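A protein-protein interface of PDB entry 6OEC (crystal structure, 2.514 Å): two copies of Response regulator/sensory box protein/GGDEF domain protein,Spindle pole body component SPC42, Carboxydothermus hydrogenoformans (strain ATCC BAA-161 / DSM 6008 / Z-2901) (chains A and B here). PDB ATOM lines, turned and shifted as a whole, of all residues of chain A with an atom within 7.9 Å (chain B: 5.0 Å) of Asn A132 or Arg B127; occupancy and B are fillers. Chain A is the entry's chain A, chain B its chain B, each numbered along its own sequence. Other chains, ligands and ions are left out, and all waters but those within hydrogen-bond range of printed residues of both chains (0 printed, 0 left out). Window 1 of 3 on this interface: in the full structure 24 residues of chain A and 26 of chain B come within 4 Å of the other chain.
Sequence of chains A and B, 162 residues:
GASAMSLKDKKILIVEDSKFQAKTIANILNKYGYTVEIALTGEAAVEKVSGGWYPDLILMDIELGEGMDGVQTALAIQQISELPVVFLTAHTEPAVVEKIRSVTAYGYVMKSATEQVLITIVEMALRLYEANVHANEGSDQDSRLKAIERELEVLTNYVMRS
The side-chain amide oxygen (OD1) of Asn A132 sits at hydrogen-bond distance from the guanidinium group (NH2) of Arg B127 (2.5 Å). OD1 of Asn A136 sits close to OE2 of Glu B123 (2.9 Å).
The side-chain amide nitrogen (ND2) of Asn A132 is in hydrogen-bond range of the side-chain hydroxyl (OH) of Tyr A106, at 3.2 Å. The backbone carbonyl oxygen of Leu A128 sits at hydrogen-bond distance from the side-chain amide nitrogen of Asn A132.
Ala A105 touches Thr B120 (CB to CG2, 3.7 Å). Met B124 touches Ala A105. Met B124 touches Leu A128 (SD to CD2, 3.5 Å). NH2 of Arg B127 touches CD2 of Leu A128, 3.9 Å away. Ala A131 touches Arg B127 (CB to NH2, 3.4 Å). Thr B120 touches Asn A132 (CG2 to ND2, 3.8 Å). Met B124 touches Asn A132 (CG to OD1, 3.7 Å). Ala A135 touches Arg B127 (CB to NH1, 3.9 Å).
Ala A125 touches none of the printed residues of chain B. Of the printed residues of chain B, Leu A128 touches Met B124 and Arg B127. Printed residues of chain B within 4 Å of Ala A131: Arg B127 (3.4 Å). Asn A132 touches three residues of chain B. Printed residues of chain B within 4 Å of Ala A135: Arg B127 (3.9 Å). Of the printed residues of chain B, Asn A136 touches Glu B123. Of the printed residues of chain A, Thr B120 touches Ala A105 (3.7 Å) and Asn A132 (3.8 Å). Of chain A, only Leu A128, Ala A131, Asn A132 and Ala A135 come within 4 Å of Arg B127. The nearest residue of chain B that does not touch Asn A132 is Glu B123 (4.2 Å). The nearest residue of chain A that does not touch Arg B127 is Asp A140 (5.7 Å).
Of the 22 printed residues of chain A, 6 touch a printed residue of chain B. Hydrophobic or aromatic side chains of chain A that line the printed part of chain B: Ala A105, Leu A128, Ala A131 and Ala A135. Of the 10 printed residues of chain B, 4 touch a printed residue of chain A. Hydrophobic or aromatic side chains of chain B within 4 Å of the printed part of chain A: Met B124.
Leu A128 touches Arg B127, but with the chains exchanged Arg A127 does not touch Leu B128 (8.6 Å). Ala A131 touches Arg B127, but with the chains exchanged Arg A127 does not touch Ala B131 (9.9 Å). Positions printed for both chains: 125, 126, 127, 128, 129, 130 and 131.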
ATOM      1  N   GLU A  82      11.285  14.361 -32.566  1.00  0.00           N
ATOM      2  CA  GLU A  82      11.314  15.460 -31.616  1.00  0.00           C
ATOM      3  C   GLU A  82      11.026  16.816 -32.275  1.00  0.00           C
ATOM      4  O   GLU A  82      11.426  17.847 -31.734  1.00  0.00           O
ATOM      5  CB  GLU A  82      12.678  15.507 -30.912  1.00  0.00           C
ATOM      6  CG  GLU A  82      13.142  14.229 -30.184  1.00  0.00           C
ATOM      7  CD  GLU A  82      14.436  14.462 -29.340  1.00  0.00           C
ATOM      8  OE1 GLU A  82      15.033  15.562 -29.431  1.00  0.00           O
ATOM      9  OE2 GLU A  82      14.864  13.552 -28.583  1.00  0.00           O
ATOM     10  N   PRO A  84       9.798  20.407 -33.533  1.00  0.00           N
ATOM     11  CA  PRO A  84       9.049  21.466 -32.847  1.00  0.00           C
ATOM     12  C   PRO A  84       7.722  21.710 -33.554  1.00  0.00           C
ATOM     13  O   PRO A  84       7.672  21.810 -34.783  1.00  0.00           O
ATOM     14  CB  PRO A  84       9.977  22.683 -32.954  1.00  0.00           C
ATOM     15  CG  PRO A  84      10.656  22.476 -34.251  1.00  0.00           C
ATOM     16  CD  PRO A  84      10.815  20.958 -34.441  1.00  0.00           C
ATOM     17  N   ALA A 105       6.042  21.957 -26.326  1.00  0.00           N
ATOM     18  CA  ALA A 105       6.767  22.926 -25.535  1.00  0.00           C
ATOM     19  C   ALA A 105       6.986  24.207 -26.302  1.00  0.00           C
ATOM     20  O   ALA A 105       7.505  25.175 -25.740  1.00  0.00           O
ATOM     21  CB  ALA A 105       8.112  22.354 -25.087  1.00  0.00           C
ATOM     22  N   TYR A 106       6.557  24.256 -27.557  1.00  0.00           N
ATOM     23  CA  TYR A 106       6.885  25.381 -28.410  1.00  0.00           C
ATOM     24  C   TYR A 106       5.747  26.372 -28.611  1.00  0.00           C
ATOM     25  O   TYR A 106       5.877  27.248 -29.467  1.00  0.00           O
ATOM     26  CB  TYR A 106       7.383  24.871 -29.756  1.00  0.00           C
ATOM     27  CG  TYR A 106       8.661  24.108 -29.613  1.00  0.00           C
ATOM     28  CD1 TYR A 106       8.644  22.765 -29.265  1.00  0.00           C
ATOM     29  CD2 TYR A 106       9.879  24.718 -29.792  1.00  0.00           C
ATOM     30  CE1 TYR A 106       9.790  22.051 -29.116  1.00  0.00           C
ATOM     31  CE2 TYR A 106      11.061  23.993 -29.654  1.00  0.00           C
ATOM     32  CZ  TYR A 106      11.003  22.660 -29.317  1.00  0.00           C
ATOM     33  OH  TYR A 106      12.157  21.909 -29.154  1.00  0.00           O
ATOM     34  N   ALA A 125      10.960  29.694 -32.190  1.00  0.00           N
ATOM     35  CA  ALA A 125      10.826  28.252 -32.048  1.00  0.00           C
ATOM     36  C   ALA A 125      11.912  27.527 -32.831  1.00  0.00           C
ATOM     37  O   ALA A 125      12.407  26.492 -32.374  1.00  0.00           O
ATOM     38  CB  ALA A 125       9.433  27.787 -32.482  1.00  0.00           C
ATOM     39  N   LEU A 126      12.323  28.071 -33.986  1.00  0.00           N
ATOM     40  CA  LEU A 126      13.392  27.441 -34.762  1.00  0.00           C
ATOM     41  C   LEU A 126      14.715  27.487 -34.022  1.00  0.00           C
ATOM     42  O   LEU A 126      15.434  26.482 -33.976  1.00  0.00           O
ATOM     43  CB  LEU A 126      13.533  28.095 -36.133  1.00  0.00           C
ATOM     44  CG  LEU A 126      12.711  27.335 -37.177  1.00  0.00           C
ATOM     45  CD1 LEU A 126      12.638  28.068 -38.498  1.00  0.00           C
ATOM     46  CD2 LEU A 126      13.281  25.933 -37.338  1.00  0.00           C
ATOM     47  N   ARG A 127      15.045  28.639 -33.421  1.00  0.00           N
ATOM     48  CA  ARG A 127      16.272  28.755 -32.630  1.00  0.00           C
ATOM     49  C   ARG A 127      16.221  27.852 -31.400  1.00  0.00           C
ATOM     50  O   ARG A 127      17.177  27.119 -31.107  1.00  0.00           O
ATOM     51  CB  ARG A 127      16.504  30.217 -32.234  1.00  0.00           C
ATOM     52  CG  ARG A 127      17.352  30.982 -33.250  1.00  0.00           C
ATOM     53  CD  ARG A 127      18.009  32.244 -32.685  1.00  0.00           C
ATOM     54  NE  ARG A 127      17.049  33.320 -32.429  1.00  0.00           N
ATOM     55  CZ  ARG A 127      16.477  33.529 -31.248  1.00  0.00           C
ATOM     56  NH1 ARG A 127      16.769  32.730 -30.227  1.00  0.00           N
ATOM     57  NH2 ARG A 127      15.624  34.533 -31.075  1.00  0.00           N
ATOM     58  N   LEU A 128      15.093  27.879 -30.686  1.00  0.00           N
ATOM     59  CA  LEU A 128      14.946  27.090 -29.473  1.00  0.00           C
ATOM     60  C   LEU A 128      15.132  25.609 -29.760  1.00  0.00           C
ATOM     61  O   LEU A 128      15.888  24.924 -29.060  1.00  0.00           O
ATOM     62  CB  LEU A 128      13.576  27.361 -28.854  1.00  0.00           C
ATOM     63  CG  LEU A 128      13.613  28.194 -27.574  1.00  0.00           C
ATOM     64  CD1 LEU A 128      12.224  28.727 -27.247  1.00  0.00           C
ATOM     65  CD2 LEU A 128      14.151  27.343 -26.437  1.00  0.00           C
ATOM     66  N   TYR A 129      14.442  25.098 -30.785  1.00  0.00           N
ATOM     67  CA  TYR A 129      14.597  23.697 -31.177  1.00  0.00           C
ATOM     68  C   TYR A 129      16.051  23.342 -31.472  1.00  0.00           C
ATOM     69  O   TYR A 129      16.527  22.271 -31.070  1.00  0.00           O
ATOM     70  CB  TYR A 129      13.742  23.407 -32.405  1.00  0.00           C
ATOM     71  CG  TYR A 129      13.942  22.033 -32.997  1.00  0.00           C
ATOM     72  CD1 TYR A 129      13.855  20.889 -32.206  1.00  0.00           C
ATOM     73  CD2 TYR A 129      14.174  21.875 -34.351  1.00  0.00           C
ATOM     74  CE1 TYR A 129      14.007  19.623 -32.760  1.00  0.00           C
ATOM     75  CE2 TYR A 129      14.321  20.630 -34.911  1.00  0.00           C
ATOM     76  CZ  TYR A 129      14.236  19.507 -34.113  1.00  0.00           C
ATOM     77  OH  TYR A 129      14.373  18.270 -34.689  1.00  0.00           O
ATOM     78  N   GLU A 130      16.761  24.211 -32.202  1.00  0.00           N
ATOM     79  CA  GLU A 130      18.160  23.939 -32.511  1.00  0.00           C
ATOM     80  C   GLU A 130      18.999  23.858 -31.242  1.00  0.00           C
ATOM     81  O   GLU A 130      19.840  22.962 -31.107  1.00  0.00           O
ATOM     82  CB  GLU A 130      18.701  24.993 -33.479  1.00  0.00           C
ATOM     83  CG  GLU A 130      17.968  24.953 -34.834  1.00  0.00           C
ATOM     84  CD  GLU A 130      18.490  25.959 -35.857  1.00  0.00           C
ATOM     85  OE1 GLU A 130      19.740  26.013 -36.047  1.00  0.00           O
ATOM     86  OE2 GLU A 130      17.644  26.683 -36.465  1.00  0.00           O
ATOM     87  N   ALA A 131      18.754  24.754 -30.283  1.00  0.00           N
ATOM     88  CA  ALA A 131      19.484  24.697 -29.017  1.00  0.00           C
ATOM     89  C   ALA A 131      19.266  23.368 -28.293  1.00  0.00           C
ATOM     90  O   ALA A 131      20.210  22.780 -27.755  1.00  0.00           O
ATOM     91  CB  ALA A 131      19.069  25.855 -28.123  1.00  0.00           C
ATOM     92  N   ASN A 132      18.028  22.881 -28.270  1.00  0.00           N
ATOM     93  CA  ASN A 132      17.750  21.650 -27.546  1.00  0.00           C
ATOM     94  C   ASN A 132      18.428  20.472 -28.223  1.00  0.00           C
ATOM     95  O   ASN A 132      18.979  19.598 -27.543  1.00  0.00           O
ATOM     96  CB  ASN A 132      16.233  21.444 -27.424  1.00  0.00           C
ATOM     97  CG  ASN A 132      15.533  22.592 -26.664  1.00  0.00           C
ATOM     98  OD1 ASN A 132      16.107  23.174 -25.739  1.00  0.00           O
ATOM     99  ND2 ASN A 132      14.289  22.907 -27.048  1.00  0.00           N
ATOM    100  N   VAL A 133      18.432  20.452 -29.563  1.00  0.00           N
ATOM    101  CA  VAL A 133      19.096  19.373 -30.297  1.00  0.00           C
ATOM    102  C   VAL A 133      20.582  19.375 -29.986  1.00  0.00           C
ATOM    103  O   VAL A 133      21.166  18.336 -29.659  1.00  0.00           O
ATOM    104  CB  VAL A 133      18.843  19.495 -31.817  1.00  0.00           C
ATOM    105  CG1 VAL A 133      19.925  18.763 -32.617  1.00  0.00           C
ATOM    106  CG2 VAL A 133      17.493  18.939 -32.189  1.00  0.00           C
ATOM    107  N   HIS A 134      21.215  20.548 -30.080  1.00  0.00           N
ATOM    108  CA  HIS A 134      22.654  20.625 -29.864  1.00  0.00           C
ATOM    109  C   HIS A 134      22.998  20.304 -28.425  1.00  0.00           C
ATOM    110  O   HIS A 134      23.943  19.551 -28.162  1.00  0.00           O
ATOM    111  CB  HIS A 134      23.181  22.008 -30.238  1.00  0.00           C
ATOM    112  CG  HIS A 134      23.057  22.333 -31.695  1.00  0.00           C
ATOM    113  ND1 HIS A 134      22.741  21.385 -32.647  1.00  0.00           N
ATOM    114  CD2 HIS A 134      23.206  23.502 -32.362  1.00  0.00           C
ATOM    115  CE1 HIS A 134      22.690  21.958 -33.836  1.00  0.00           C
ATOM    116  NE2 HIS A 134      22.976  23.240 -33.692  1.00  0.00           N
ATOM    117  N   ALA A 135      22.230  20.852 -27.478  1.00  0.00           N
ATOM    118  CA  ALA A 135      22.483  20.578 -26.068  1.00  0.00           C
ATOM    119  C   ALA A 135      22.369  19.089 -25.763  1.00  0.00           C
ATOM    120  O   ALA A 135      23.188  18.535 -25.017  1.00  0.00           O
ATOM    121  CB  ALA A 135      21.519  21.376 -25.203  1.00  0.00           C
ATOM    122  N   ASN A 136      21.382  18.417 -26.354  1.00  0.00           N
ATOM    123  CA  ASN A 136      21.178  17.005 -26.046  1.00  0.00           C
ATOM    124  C   ASN A 136      22.231  16.102 -26.694  1.00  0.00           C
ATOM    125  O   ASN A 136      22.496  15.005 -26.180  1.00  0.00           O
ATOM    126  CB  ASN A 136      19.750  16.586 -26.437  1.00  0.00           C
ATOM    127  CG  ASN A 136      18.726  16.877 -25.320  1.00  0.00           C
ATOM    128  OD1 ASN A 136      19.064  17.452 -24.268  1.00  0.00           O
ATOM    129  ND2 ASN A 136      17.479  16.478 -25.546  1.00  0.00           N
ATOM    130  N   GLU A 137      22.854  16.539 -27.785  1.00  0.00           N
ATOM    131  CA  GLU A 137      23.970  15.813 -28.373  1.00  0.00           C
ATOM    132  C   GLU A 137      25.312  16.457 -28.040  1.00  0.00           C
ATOM    133  O   GLU A 137      26.343  16.024 -28.563  1.00  0.00           O
ATOM    134  CB  GLU A 137      23.794  15.689 -29.893  1.00  0.00           C
ATOM    135  CG  GLU A 137      24.145  16.950 -30.661  1.00  0.00           C
ATOM    136  CD  GLU A 137      23.749  16.894 -32.135  1.00  0.00           C
ATOM    137  OE1 GLU A 137      22.952  16.000 -32.511  1.00  0.00           O
ATOM    138  OE2 GLU A 137      24.236  17.753 -32.921  1.00  0.00           O
ATOM    139  N   GLY A 138      25.324  17.477 -27.181  1.00  0.00           N
ATOM    140  CA  GLY A 138      26.555  18.097 -26.741  1.00  0.00           C
ATOM    141  C   GLY A 138      27.104  19.196 -27.629  1.00  0.00           C
ATOM    142  O   GLY A 138      27.971  19.956 -27.174  1.00  0.00           O
ATOM    143  N   SER A 139      26.623  19.328 -28.868  1.00  0.00           N
ATOM    144  CA  SER A 139      27.243  20.217 -29.849  1.00  0.00           C
ATOM    145  C   SER A 139      26.836  21.679 -29.701  1.00  0.00           C
ATOM    146  O   SER A 139      27.019  22.448 -30.652  1.00  0.00           O
ATOM    147  CB  SER A 139      26.932  19.744 -31.274  1.00  0.00           C
ATOM    148  OG  SER A 139      25.630  20.123 -31.681  1.00  0.00           O
ATOM    149  N   ASP A 140      26.304  22.098 -28.559  1.00  0.00           N
ATOM    150  CA  ASP A 140      25.917  23.494 -28.438  1.00  0.00           C
ATOM    151  C   ASP A 140      27.145  24.382 -28.220  1.00  0.00           C
ATOM    152  O   ASP A 140      28.212  23.930 -27.794  1.00  0.00           O
ATOM    153  CB  ASP A 140      24.920  23.676 -27.297  1.00  0.00           C
ATOM    154  CG  ASP A 140      25.518  23.343 -25.952  1.00  0.00           C
ATOM    155  OD1 ASP A 140      25.882  22.160 -25.744  1.00  0.00           O
ATOM    156  OD2 ASP A 140      25.649  24.275 -25.123  1.00  0.00           O
ATOM    157  N   ASP A 142      27.653  26.882 -26.081  1.00  0.00           N
ATOM    158  CA  ASP A 142      28.062  27.096 -24.694  1.00  0.00           C
ATOM    159  C   ASP A 142      28.978  25.972 -24.205  1.00  0.00           C
ATOM    160  O   ASP A 142      29.986  26.228 -23.531  1.00  0.00           O
ATOM    161  CB  ASP A 142      26.829  27.224 -23.788  1.00  0.00           C
ATOM    162  CG  ASP A 142      27.069  28.143 -22.584  1.00  0.00           C
ATOM    163  OD1 ASP A 142      27.033  29.387 -22.755  1.00  0.00           O
ATOM    164  OD2 ASP A 142      27.295  27.623 -21.466  1.00  0.00           O
ATOM    165  N   SER A 143      28.645  24.721 -24.539  1.00  0.00           N
ATOM    166  CA  SER A 143      29.452  23.588 -24.097  1.00  0.00           C
ATOM    167  C   SER A 143      30.833  23.620 -24.732  1.00  0.00           C
ATOM    168  O   SER A 143      31.851  23.590 -24.028  1.00  0.00           O
ATOM    169  CB  SER A 143      28.742  22.282 -24.431  1.00  0.00           C
ATOM    170  OG  SER A 143      27.517  22.190 -23.734  1.00  0.00           O
ATOM    171  N   THR B 120      11.454  18.916 -22.016  1.00  0.00           N
ATOM    172  CA  THR B 120      11.879  20.022 -22.863  1.00  0.00           C
ATOM    173  C   THR B 120      11.627  21.333 -22.162  1.00  0.00           C
ATOM    174  O   THR B 120      12.442  22.261 -22.262  1.00  0.00           O
ATOM    175  CB  THR B 120      11.156  19.968 -24.213  1.00  0.00           C
ATOM    176  OG1 THR B 120      11.480  18.737 -24.863  1.00  0.00           O
ATOM    177  CG2 THR B 120      11.554  21.128 -25.131  1.00  0.00           C
ATOM    178  N   GLU B 123      14.610  21.343 -19.558  1.00  0.00           N
ATOM    179  CA  GLU B 123      15.809  21.771 -20.296  1.00  0.00           C
ATOM    180  C   GLU B 123      15.752  23.249 -20.675  1.00  0.00           C
ATOM    181  O   GLU B 123      16.717  23.997 -20.455  1.00  0.00           O
ATOM    182  CB  GLU B 123      16.008  20.955 -21.578  1.00  0.00           C
ATOM    183  CG  GLU B 123      16.500  19.541 -21.391  1.00  0.00           C
ATOM    184  CD  GLU B 123      16.402  18.720 -22.694  1.00  0.00           C
ATOM    185  OE1 GLU B 123      16.073  19.333 -23.757  1.00  0.00           O
ATOM    186  OE2 GLU B 123      16.647  17.471 -22.647  1.00  0.00           O
ATOM    187  N   MET B 124      14.633  23.684 -21.279  1.00  0.00           N
ATOM    188  CA  MET B 124      14.544  25.073 -21.715  1.00  0.00           C
ATOM    189  C   MET B 124      14.630  26.031 -20.544  1.00  0.00           C
ATOM    190  O   MET B 124      15.240  27.098 -20.668  1.00  0.00           O
ATOM    191  CB  MET B 124      13.268  25.314 -22.511  1.00  0.00           C
ATOM    192  CG  MET B 124      13.332  24.689 -23.883  1.00  0.00           C
ATOM    193  SD  MET B 124      11.947  25.064 -24.970  1.00  0.00           S
ATOM    194  CE  MET B 124      10.598  25.012 -23.827  1.00  0.00           C
ATOM    195  N   ALA B 125      14.054  25.667 -19.395  1.00  0.00           N
ATOM    196  CA  ALA B 125      14.116  26.555 -18.238  1.00  0.00           C
ATOM    197  C   ALA B 125      15.530  26.636 -17.693  1.00  0.00           C
ATOM    198  O   ALA B 125      15.980  27.702 -17.257  1.00  0.00           O
ATOM    199  CB  ALA B 125      13.167  26.078 -17.148  1.00  0.00           C
ATOM    200  N   LEU B 126      16.239  25.512 -17.724  1.00  0.00           N
ATOM    201  CA  LEU B 126      17.614  25.487 -17.264  1.00  0.00           C
ATOM    202  C   LEU B 126      18.509  26.389 -18.119  1.00  0.00           C
ATOM    203  O   LEU B 126      19.322  27.145 -17.579  1.00  0.00           O
ATOM    204  CB  LEU B 126      18.112  24.040 -17.227  1.00  0.00           C
ATOM    205  CG  LEU B 126      17.605  23.225 -16.034  1.00  0.00           C
ATOM    206  CD1 LEU B 126      17.760  21.738 -16.225  1.00  0.00           C
ATOM    207  CD2 LEU B 126      18.348  23.630 -14.786  1.00  0.00           C
ATOM    208  N   ARG B 127      18.354  26.364 -19.447  1.00  0.00           N
ATOM    209  CA  ARG B 127      19.229  27.205 -20.275  1.00  0.00           C
ATOM    210  C   ARG B 127      18.838  28.681 -20.220  1.00  0.00           C
ATOM    211  O   ARG B 127      19.706  29.555 -20.313  1.00  0.00           O
ATOM    212  CB  ARG B 127      19.249  26.712 -21.720  1.00  0.00           C
ATOM    213  CG  ARG B 127      20.094  25.466 -21.890  1.00  0.00           C
ATOM    214  CD  ARG B 127      20.351  25.186 -23.347  1.00  0.00           C
ATOM    215  NE  ARG B 127      19.214  25.621 -24.141  1.00  0.00           N
ATOM    216  CZ  ARG B 127      18.257  24.815 -24.598  1.00  0.00           C
ATOM    217  NH1 ARG B 127      18.304  23.496 -24.345  1.00  0.00           N
ATOM    218  NH2 ARG B 127      17.255  25.338 -25.324  1.00  0.00           N
ATOM    219  N   LEU B 128      17.552  28.975 -20.065  1.00  0.00           N
ATOM    220  CA  LEU B 128      17.113  30.343 -19.805  1.00  0.00           C
ATOM    221  C   LEU B 128      17.807  30.929 -18.580  1.00  0.00           C
ATOM    222  O   LEU B 128      18.337  32.045 -18.619  1.00  0.00           O
ATOM    223  CB  LEU B 128      15.605  30.345 -19.594  1.00  0.00           C
ATOM    224  CG  LEU B 128      14.816  31.275 -20.483  1.00  0.00           C
ATOM    225  CD1 LEU B 128      14.778  32.536 -19.749  1.00  0.00           C
ATOM    226  CD2 LEU B 128      15.525  31.445 -21.818  1.00  0.00           C
ATOM    227  N   TYR B 129      17.791  30.191 -17.473  1.00  0.00           N
ATOM    228  CA  TYR B 129      18.399  30.672 -16.239  1.00  0.00           C
ATOM    229  C   TYR B 129      19.905  30.848 -16.400  1.00  0.00           C
ATOM    230  O   TYR B 129      20.461  31.881 -16.013  1.00  0.00           O
ATOM    231  CB  TYR B 129      18.078  29.705 -15.107  1.00  0.00           C
ATOM    232  CG  TYR B 129      18.777  30.035 -13.830  1.00  0.00           C
ATOM    233  CD1 TYR B 129      18.233  30.966 -12.941  1.00  0.00           C
ATOM    234  CD2 TYR B 129      19.977  29.414 -13.497  1.00  0.00           C
ATOM    235  CE1 TYR B 129      18.876  31.271 -11.753  1.00  0.00           C
ATOM    236  CE2 TYR B 129      20.613  29.697 -12.324  1.00  0.00           C
ATOM    237  CZ  TYR B 129      20.072  30.632 -11.454  1.00  0.00           C
ATOM    238  OH  TYR B 129      20.733  30.929 -10.284  1.00  0.00           O
ATOM    239  N   GLU B 130      20.578  29.849 -16.985  1.00  0.00           N
ATOM    240  CA  GLU B 130      21.995  29.994 -17.329  1.00  0.00           C
ATOM    241  C   GLU B 130      22.252  31.228 -18.186  1.00  0.00           C
ATOM    242  O   GLU B 130      23.278  31.899 -18.024  1.00  0.00           O
ATOM    243  CB  GLU B 130      22.497  28.746 -18.052  1.00  0.00           C
ATOM    244  CG  GLU B 130      23.358  27.839 -17.187  1.00  0.00           C
ATOM    245  CD  GLU B 130      22.956  26.386 -17.337  1.00  0.00           C
ATOM    246  OE1 GLU B 130      22.736  25.972 -18.506  1.00  0.00           O
ATOM    247  OE2 GLU B 130      22.830  25.683 -16.293  1.00  0.00           O
ATOM    248  N   ALA B 131      21.339  31.543 -19.107  1.00  0.00           N
ATOM    249  CA  ALA B 131      21.494  32.759 -19.896  1.00  0.00           C
ATOM    250  C   ALA B 131      21.417  34.002 -19.022  1.00  0.00           C
ATOM    251  O   ALA B 131      22.189  34.940 -19.209  1.00  0.00           O
ATOM    252  CB  ALA B 131      20.442  32.818 -20.993  1.00  0.00           C
